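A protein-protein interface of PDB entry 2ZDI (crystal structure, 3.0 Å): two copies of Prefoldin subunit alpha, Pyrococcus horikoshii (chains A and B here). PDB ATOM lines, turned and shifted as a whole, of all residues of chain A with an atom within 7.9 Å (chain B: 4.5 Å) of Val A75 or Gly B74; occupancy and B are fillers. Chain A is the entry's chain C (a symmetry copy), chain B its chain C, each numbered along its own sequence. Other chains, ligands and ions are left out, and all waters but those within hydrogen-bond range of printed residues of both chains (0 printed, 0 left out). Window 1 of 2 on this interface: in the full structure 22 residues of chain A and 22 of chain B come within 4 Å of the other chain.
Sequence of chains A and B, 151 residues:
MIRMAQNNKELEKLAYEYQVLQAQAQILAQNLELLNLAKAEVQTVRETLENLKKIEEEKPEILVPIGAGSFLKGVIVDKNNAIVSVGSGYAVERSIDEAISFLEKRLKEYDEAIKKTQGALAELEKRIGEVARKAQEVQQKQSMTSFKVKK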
ATOM      1  N   GLU A  58     -12.282 -17.093   2.328  1.00  0.00           N
ATOM      2  CA  GLU A  58     -11.550 -17.651   1.193  1.00  0.00           C
ATOM      3  C   GLU A  58     -10.135 -17.072   1.033  1.00  0.00           C
ATOM      4  O   GLU A  58      -9.170 -17.594   1.602  1.00  0.00           O
ATOM      5  CB  GLU A  58     -12.382 -17.450  -0.073  1.00  0.00           C
ATOM      6  CG  GLU A  58     -13.679 -16.709   0.164  1.00  0.00           C
ATOM      7  CD  GLU A  58     -13.765 -15.452  -0.671  1.00  0.00           C
ATOM      8  OE1 GLU A  58     -12.902 -15.272  -1.560  1.00  0.00           O
ATOM      9  OE2 GLU A  58     -14.686 -14.642  -0.430  1.00  0.00           O
ATOM     10  N   LYS A  59     -10.021 -15.997   0.253  1.00  0.00           N
ATOM     11  CA  LYS A  59      -8.776 -15.241   0.148  1.00  0.00           C
ATOM     12  C   LYS A  59      -8.958 -13.893   0.845  1.00  0.00           C
ATOM     13  O   LYS A  59      -9.475 -12.948   0.243  1.00  0.00           O
ATOM     14  CB  LYS A  59      -8.377 -15.043  -1.311  1.00  0.00           C
ATOM     15  CG  LYS A  59      -8.096 -16.332  -2.061  1.00  0.00           C
ATOM     16  CD  LYS A  59      -7.702 -16.030  -3.495  1.00  0.00           C
ATOM     17  CE  LYS A  59      -7.548 -17.291  -4.325  1.00  0.00           C
ATOM     18  NZ  LYS A  59      -7.186 -16.932  -5.722  1.00  0.00           N
ATOM     19  N   PRO A  60      -8.552 -13.812   2.105  1.00  0.00           N
ATOM     20  CA  PRO A  60      -8.752 -12.674   3.013  1.00  0.00           C
ATOM     21  C   PRO A  60      -8.141 -11.363   2.520  1.00  0.00           C
ATOM     22  O   PRO A  60      -6.997 -11.330   2.066  1.00  0.00           O
ATOM     23  CB  PRO A  60      -8.065 -13.121   4.302  1.00  0.00           C
ATOM     24  CG  PRO A  60      -8.111 -14.606   4.255  1.00  0.00           C
ATOM     25  CD  PRO A  60      -7.934 -14.958   2.817  1.00  0.00           C
ATOM     26  N   GLU A  61      -8.922 -10.292   2.625  1.00  0.00           N
ATOM     27  CA  GLU A  61      -8.450  -8.949   2.324  1.00  0.00           C
ATOM     28  C   GLU A  61      -7.682  -8.402   3.519  1.00  0.00           C
ATOM     29  O   GLU A  61      -8.094  -8.581   4.664  1.00  0.00           O
ATOM     30  CB  GLU A  61      -9.626  -8.025   2.007  1.00  0.00           C
ATOM     31  CG  GLU A  61     -10.591  -8.563   0.961  1.00  0.00           C
ATOM     32  CD  GLU A  61     -11.478  -7.476   0.383  1.00  0.00           C
ATOM     33  OE1 GLU A  61     -11.091  -6.291   0.460  1.00  0.00           O
ATOM     34  OE2 GLU A  61     -12.558  -7.806  -0.152  1.00  0.00           O
ATOM     35  N   ILE A  62      -6.570  -7.727   3.246  1.00  0.00           N
ATOM     36  CA  ILE A  62      -5.701  -7.216   4.296  1.00  0.00           C
ATOM     37  C   ILE A  62      -5.176  -5.821   3.972  1.00  0.00           C
ATOM     38  O   ILE A  62      -5.241  -5.369   2.830  1.00  0.00           O
ATOM     39  CB  ILE A  62      -4.483  -8.141   4.503  1.00  0.00           C
ATOM     40  CG1 ILE A  62      -3.768  -8.372   3.173  1.00  0.00           C
ATOM     41  CG2 ILE A  62      -4.904  -9.471   5.091  1.00  0.00           C
ATOM     42  CD1 ILE A  62      -2.376  -8.909   3.322  1.00  0.00           C
ATOM     43  N   LEU A  63      -4.660  -5.145   4.991  1.00  0.00           N
ATOM     44  CA  LEU A  63      -3.862  -3.941   4.793  1.00  0.00           C
ATOM     45  C   LEU A  63      -2.412  -4.280   5.085  1.00  0.00           C
ATOM     46  O   LEU A  63      -2.077  -4.699   6.196  1.00  0.00           O
ATOM     47  CB  LEU A  63      -4.323  -2.808   5.710  1.00  0.00           C
ATOM     48  CG  LEU A  63      -5.323  -1.820   5.114  1.00  0.00           C
ATOM     49  CD1 LEU A  63      -6.324  -2.544   4.241  1.00  0.00           C
ATOM     50  CD2 LEU A  63      -6.021  -1.041   6.213  1.00  0.00           C
ATOM     51  N   VAL A  64      -1.554  -4.122   4.083  1.00  0.00           N
ATOM     52  CA  VAL A  64      -0.131  -4.382   4.262  1.00  0.00           C
ATOM     53  C   VAL A  64       0.623  -3.104   4.626  1.00  0.00           C
ATOM     54  O   VAL A  64       0.668  -2.152   3.837  1.00  0.00           O
ATOM     55  CB  VAL A  64       0.495  -5.087   3.031  1.00  0.00           C
ATOM     56  CG1 VAL A  64      -0.335  -4.834   1.780  1.00  0.00           C
ATOM     57  CG2 VAL A  64       1.949  -4.665   2.839  1.00  0.00           C
ATOM     58  N   LEU A  72      -1.104  -0.528   2.156  1.00  0.00           N
ATOM     59  CA  LEU A  72      -1.577  -0.832   0.821  1.00  0.00           C
ATOM     60  C   LEU A  72      -2.686  -1.866   0.929  1.00  0.00           C
ATOM     61  O   LEU A  72      -2.790  -2.578   1.928  1.00  0.00           O
ATOM     62  CB  LEU A  72      -0.435  -1.334  -0.067  1.00  0.00           C
ATOM     63  CG  LEU A  72       0.705  -0.356  -0.371  1.00  0.00           C
ATOM     64  CD1 LEU A  72       1.669  -0.985  -1.345  1.00  0.00           C
ATOM     65  CD2 LEU A  72       0.187   0.961  -0.928  1.00  0.00           C
ATOM     66  N   LYS A  73      -3.527  -1.931  -0.096  1.00  0.00           N
ATOM     67  CA  LYS A  73      -4.662  -2.836  -0.074  1.00  0.00           C
ATOM     68  C   LYS A  73      -4.279  -4.120  -0.799  1.00  0.00           C
ATOM     69  O   LYS A  73      -3.818  -4.081  -1.943  1.00  0.00           O
ATOM     70  CB  LYS A  73      -5.881  -2.167  -0.722  1.00  0.00           C
ATOM     71  CG  LYS A  73      -7.157  -2.223   0.117  1.00  0.00           C
ATOM     72  CD  LYS A  73      -8.117  -1.086  -0.252  1.00  0.00           C
ATOM     73  CE  LYS A  73      -9.246  -0.911   0.778  1.00  0.00           C
ATOM     74  NZ  LYS A  73     -10.455  -1.770   0.552  1.00  0.00           N
ATOM     75  N   GLY A  74      -4.446  -5.253  -0.124  1.00  0.00           N
ATOM     76  CA  GLY A  74      -4.119  -6.539  -0.708  1.00  0.00           C
ATOM     77  C   GLY A  74      -5.021  -7.677  -0.263  1.00  0.00           C
ATOM     78  O   GLY A  74      -6.037  -7.471   0.398  1.00  0.00           O
ATOM     79  N   VAL A  75      -4.641  -8.890  -0.640  1.00  0.00           N
ATOM     80  CA  VAL A  75      -5.367 -10.090  -0.251  1.00  0.00           C
ATOM     81  C   VAL A  75      -4.381 -11.245  -0.106  1.00  0.00           C
ATOM     82  O   VAL A  75      -3.468 -11.391  -0.921  1.00  0.00           O
ATOM     83  CB  VAL A  75      -6.424 -10.459  -1.304  1.00  0.00           C
ATOM     84  CG1 VAL A  75      -5.897 -10.158  -2.693  1.00  0.00           C
ATOM     85  CG2 VAL A  75      -6.820 -11.928  -1.182  1.00  0.00           C
ATOM     86  N   ILE A  76      -4.549 -12.057   0.932  1.00  0.00           N
ATOM     87  CA  ILE A  76      -3.664 -13.198   1.123  1.00  0.00           C
ATOM     88  C   ILE A  76      -4.147 -14.401   0.305  1.00  0.00           C
ATOM     89  O   ILE A  76      -5.221 -14.948   0.549  1.00  0.00           O
ATOM     90  CB  ILE A  76      -3.463 -13.539   2.616  1.00  0.00           C
ATOM     91  CG1 ILE A  76      -4.764 -13.973   3.266  1.00  0.00           C
ATOM     92  CG2 ILE A  76      -2.958 -12.330   3.371  1.00  0.00           C
ATOM     93  CD1 ILE A  76      -4.717 -13.858   4.772  1.00  0.00           C
ATOM     94  N   VAL A  77      -3.340 -14.793  -0.678  1.00  0.00           N
ATOM     95  CA  VAL A  77      -3.764 -15.754  -1.694  1.00  0.00           C
ATOM     96  C   VAL A  77      -3.643 -17.225  -1.283  1.00  0.00           C
ATOM     97  O   VAL A  77      -4.466 -18.052  -1.679  1.00  0.00           O
ATOM     98  CB  VAL A  77      -3.020 -15.524  -3.018  1.00  0.00           C
ATOM     99  CG1 VAL A  77      -3.189 -14.088  -3.458  1.00  0.00           C
ATOM    100  CG2 VAL A  77      -1.553 -15.856  -2.863  1.00  0.00           C
ATOM    101  N   ASP A  78      -2.621 -17.558  -0.502  1.00  0.00           N
ATOM    102  CA  ASP A  78      -2.512 -18.909   0.035  1.00  0.00           C
ATOM    103  C   ASP A  78      -2.603 -18.886   1.558  1.00  0.00           C
ATOM    104  O   ASP A  78      -1.593 -18.937   2.261  1.00  0.00           O
ATOM    105  CB  ASP A  78      -1.228 -19.600  -0.429  1.00  0.00           C
ATOM    106  CG  ASP A  78      -1.282 -21.111  -0.262  1.00  0.00           C
ATOM    107  OD1 ASP A  78      -2.371 -21.641   0.061  1.00  0.00           O
ATOM    108  OD2 ASP A  78      -0.239 -21.771  -0.456  1.00  0.00           O
ATOM    109  N   LYS A  79      -3.831 -18.802   2.056  1.00  0.00           N
ATOM    110  CA  LYS A  79      -4.092 -18.762   3.487  1.00  0.00           C
ATOM    111  C   LYS A  79      -3.705 -20.078   4.166  1.00  0.00           C
ATOM    112  O   LYS A  79      -3.627 -20.160   5.393  1.00  0.00           O
ATOM    113  CB  LYS A  79      -5.570 -18.421   3.730  1.00  0.00           C
ATOM    114  CG  LYS A  79      -6.197 -19.062   4.958  1.00  0.00           C
ATOM    115  CD  LYS A  79      -7.658 -18.670   5.106  1.00  0.00           C
ATOM    116  CE  LYS A  79      -8.436 -19.735   5.863  1.00  0.00           C
ATOM    117  NZ  LYS A  79      -7.724 -20.206   7.085  1.00  0.00           N
ATOM    118  N   PRO B  60       0.363  -6.866  -8.536  1.00  0.00           N
ATOM    119  CA  PRO B  60       1.660  -7.443  -8.157  1.00  0.00           C
ATOM    120  C   PRO B  60       1.583  -8.481  -7.039  1.00  0.00           C
ATOM    121  O   PRO B  60       0.918  -8.270  -6.025  1.00  0.00           O
ATOM    122  CB  PRO B  60       2.468  -6.232  -7.695  1.00  0.00           C
ATOM    123  CG  PRO B  60       1.862  -5.081  -8.413  1.00  0.00           C
ATOM    124  CD  PRO B  60       0.403  -5.384  -8.477  1.00  0.00           C
ATOM    125  N   GLU B  61       2.281  -9.594  -7.242  1.00  0.00           N
ATOM    126  CA  GLU B  61       2.421 -10.625  -6.223  1.00  0.00           C
ATOM    127  C   GLU B  61       3.511 -10.222  -5.241  1.00  0.00           C
ATOM    128  O   GLU B  61       4.560  -9.718  -5.641  1.00  0.00           O
ATOM    129  CB  GLU B  61       2.780 -11.967  -6.863  1.00  0.00           C
ATOM    130  CG  GLU B  61       1.873 -12.385  -8.011  1.00  0.00           C
ATOM    131  CD  GLU B  61       1.994 -13.863  -8.329  1.00  0.00           C
ATOM    132  OE1 GLU B  61       2.429 -14.629  -7.443  1.00  0.00           O
ATOM    133  OE2 GLU B  61       1.650 -14.262  -9.463  1.00  0.00           O
ATOM    134  N   ILE B  62       3.262 -10.455  -3.957  1.00  0.00           N
ATOM    135  CA  ILE B  62       4.186 -10.050  -2.907  1.00  0.00           C
ATOM    136  C   ILE B  62       4.313 -11.112  -1.819  1.00  0.00           C
ATOM    137  O   ILE B  62       3.488 -12.019  -1.719  1.00  0.00           O
ATOM    138  CB  ILE B  62       3.719  -8.742  -2.235  1.00  0.00           C
ATOM    139  CG1 ILE B  62       2.273  -8.884  -1.760  1.00  0.00           C
ATOM    140  CG2 ILE B  62       3.827  -7.572  -3.190  1.00  0.00           C
ATOM    141  CD1 ILE B  62       1.862  -7.845  -0.759  1.00  0.00           C
ATOM    142  N   LEU B  72       3.772 -14.600   4.133  1.00  0.00           N
ATOM    143  CA  LEU B  72       2.580 -15.147   3.518  1.00  0.00           C
ATOM    144  C   LEU B  72       2.542 -14.700   2.066  1.00  0.00           C
ATOM    145  O   LEU B  72       3.179 -13.715   1.692  1.00  0.00           O
ATOM    146  CB  LEU B  72       1.321 -14.705   4.268  1.00  0.00           C
ATOM    147  CG  LEU B  72       1.156 -15.185   5.715  1.00  0.00           C
ATOM    148  CD1 LEU B  72      -0.187 -14.750   6.245  1.00  0.00           C
ATOM    149  CD2 LEU B  72       1.296 -16.695   5.829  1.00  0.00           C
ATOM    150  N   LYS B  73       1.807 -15.440   1.245  1.00  0.00           N
ATOM    151  CA  LYS B  73       1.749 -15.145  -0.176  1.00  0.00           C
ATOM    152  C   LYS B  73       0.513 -14.297  -0.449  1.00  0.00           C
ATOM    153  O   LYS B  73      -0.601 -14.670  -0.069  1.00  0.00           O
ATOM    154  CB  LYS B  73       1.725 -16.449  -0.983  1.00  0.00           C
ATOM    155  CG  LYS B  73       2.757 -16.518  -2.108  1.00  0.00           C
ATOM    156  CD  LYS B  73       3.101 -17.970  -2.461  1.00  0.00           C
ATOM    157  CE  LYS B  73       4.356 -18.081  -3.341  1.00  0.00           C
ATOM    158  NZ  LYS B  73       4.113 -17.964  -4.818  1.00  0.00           N
ATOM    159  N   GLY B  74       0.714 -13.147  -1.084  1.00  0.00           N
ATOM    160  CA  GLY B  74      -0.384 -12.254  -1.403  1.00  0.00           C
ATOM    161  C   GLY B  74      -0.212 -11.490  -2.704  1.00  0.00           C
ATOM    162  O   GLY B  74       0.700 -11.749  -3.486  1.00  0.00           O
ATOM    163  N   VAL B  75      -1.110 -10.542  -2.933  1.00  0.00           N
ATOM    164  CA  VAL B  75      -1.055  -9.684  -4.109  1.00  0.00           C
ATOM    165  C   VAL B  75      -1.612  -8.310  -3.750  1.00  0.00           C
ATOM    166  O   VAL B  75      -2.613  -8.209  -3.039  1.00  0.00           O
ATOM    167  CB  VAL B  75      -1.880 -10.278  -5.261  1.00  0.00           C
ATOM    168  CG1 VAL B  75      -3.126 -10.946  -4.714  1.00  0.00           C
ATOM    169  CG2 VAL B  75      -2.247  -9.199  -6.276  1.00  0.00           C
ATOM    170  N   VAL B  77      -3.748  -5.322  -4.462  1.00  0.00           N
ATOM    171  CA  VAL B  77      -4.923  -5.178  -5.319  1.00  0.00           C
ATOM    172  C   VAL B  77      -5.157  -3.765  -5.863  1.00  0.00           C
ATOM    173  O   VAL B  77      -5.632  -3.602  -6.988  1.00  0.00           O
ATOM    174  CB  VAL B  77      -6.190  -5.676  -4.608  1.00  0.00           C
ATOM    175  CG1 VAL B  77      -5.984  -7.092  -4.125  1.00  0.00           C
ATOM    176  CG2 VAL B  77      -6.535  -4.770  -3.447  1.00  0.00           C
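Lys A73 touches Val B77, and with the chains exchanged Val A77 touches Lys B73.
Gly A74 touches Val B77, and with the chains exchanged Val A77 touches Gly B74.
Val B75 touches its own counterpart, Val A75.
Val A75 touches Val B77, and with the chains exchanged Val A77 touches Val B75.
8 positions are printed for both chains.
O of Val B75 touches CA of Gly A74 (3.2 Å).
Gly A74 touches Val B77 (CA to CG1, 3.9 Å).
Gly B74 touches Val A75.
Val A75 touches Val B77 (CG1 to CG1, 3.4 Å).
Lys B73 touches Ile A76.
Val A77 touches Gly B74 (CG1 to CA, 3.9 Å).
CG1 of Val A77 touches CG1 of Val B75 (3.4 Å).
N of Asp A78 touches O of Lys B73 (3.6 Å).
Hydrophobic or aromatic side chains of chain B within 4 Å of the printed part of chain A: Val B75 and Val B77.
Printed residues of chain A that touch a printed residue of chain B: Lys A73, Gly A74, Val A75, Ile A76, Val A77 and Asp A78.
Among the printed residues, 11 pairs touch across the chains.
The backbone carbonyl oxygen of Val A75 lies within hydrogen-bond range of the backbone NH of Val B75 (3.2 Å).
The backbone NH (N) of Val B77 sits at hydrogen-bond distance from the backbone carbonyl oxygen (O) of Lys A73 (2.8 Å).
The backbone carbonyl oxygen (O) of Lys B73 lies within hydrogen-bond range of the backbone NH (N) of Val A77, 2.8 Å away.
The backbone carbonyl oxygen (O) of Pro A60 is in hydrogen-bond range of the backbone NH (N) of Ile A76 (2.8 Å).
The backbone NH (N) of Ile B62 is in hydrogen-bond range of the backbone carbonyl oxygen (O) of Gly B74.
The backbone NH (N) of Ile A62 sits at hydrogen-bond distance from the backbone carbonyl oxygen (O) of Gly A74.
Val A75 touches just these residues of chain B: Gly B74, Val B75 and Val B77.
Of the printed residues of chain B, Lys A73 touches Val B77.
Printed residues of chain A within 4 Å of Lys B73: Ile A76, Val A77 and Asp A78.
Of the printed residues of chain A, Val B77 touches Lys A73 (2.8 Å), Gly A74 (3.9 Å) and Val A75 (3.4 Å).
Of the printed residues of chain B, Gly A74 touches Val B75 (3.2 Å) and Val B77 (3.9 Å).
The nearest printed residue of chain B that does not touch Val A77 is Glu B61 (6.2 Å).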
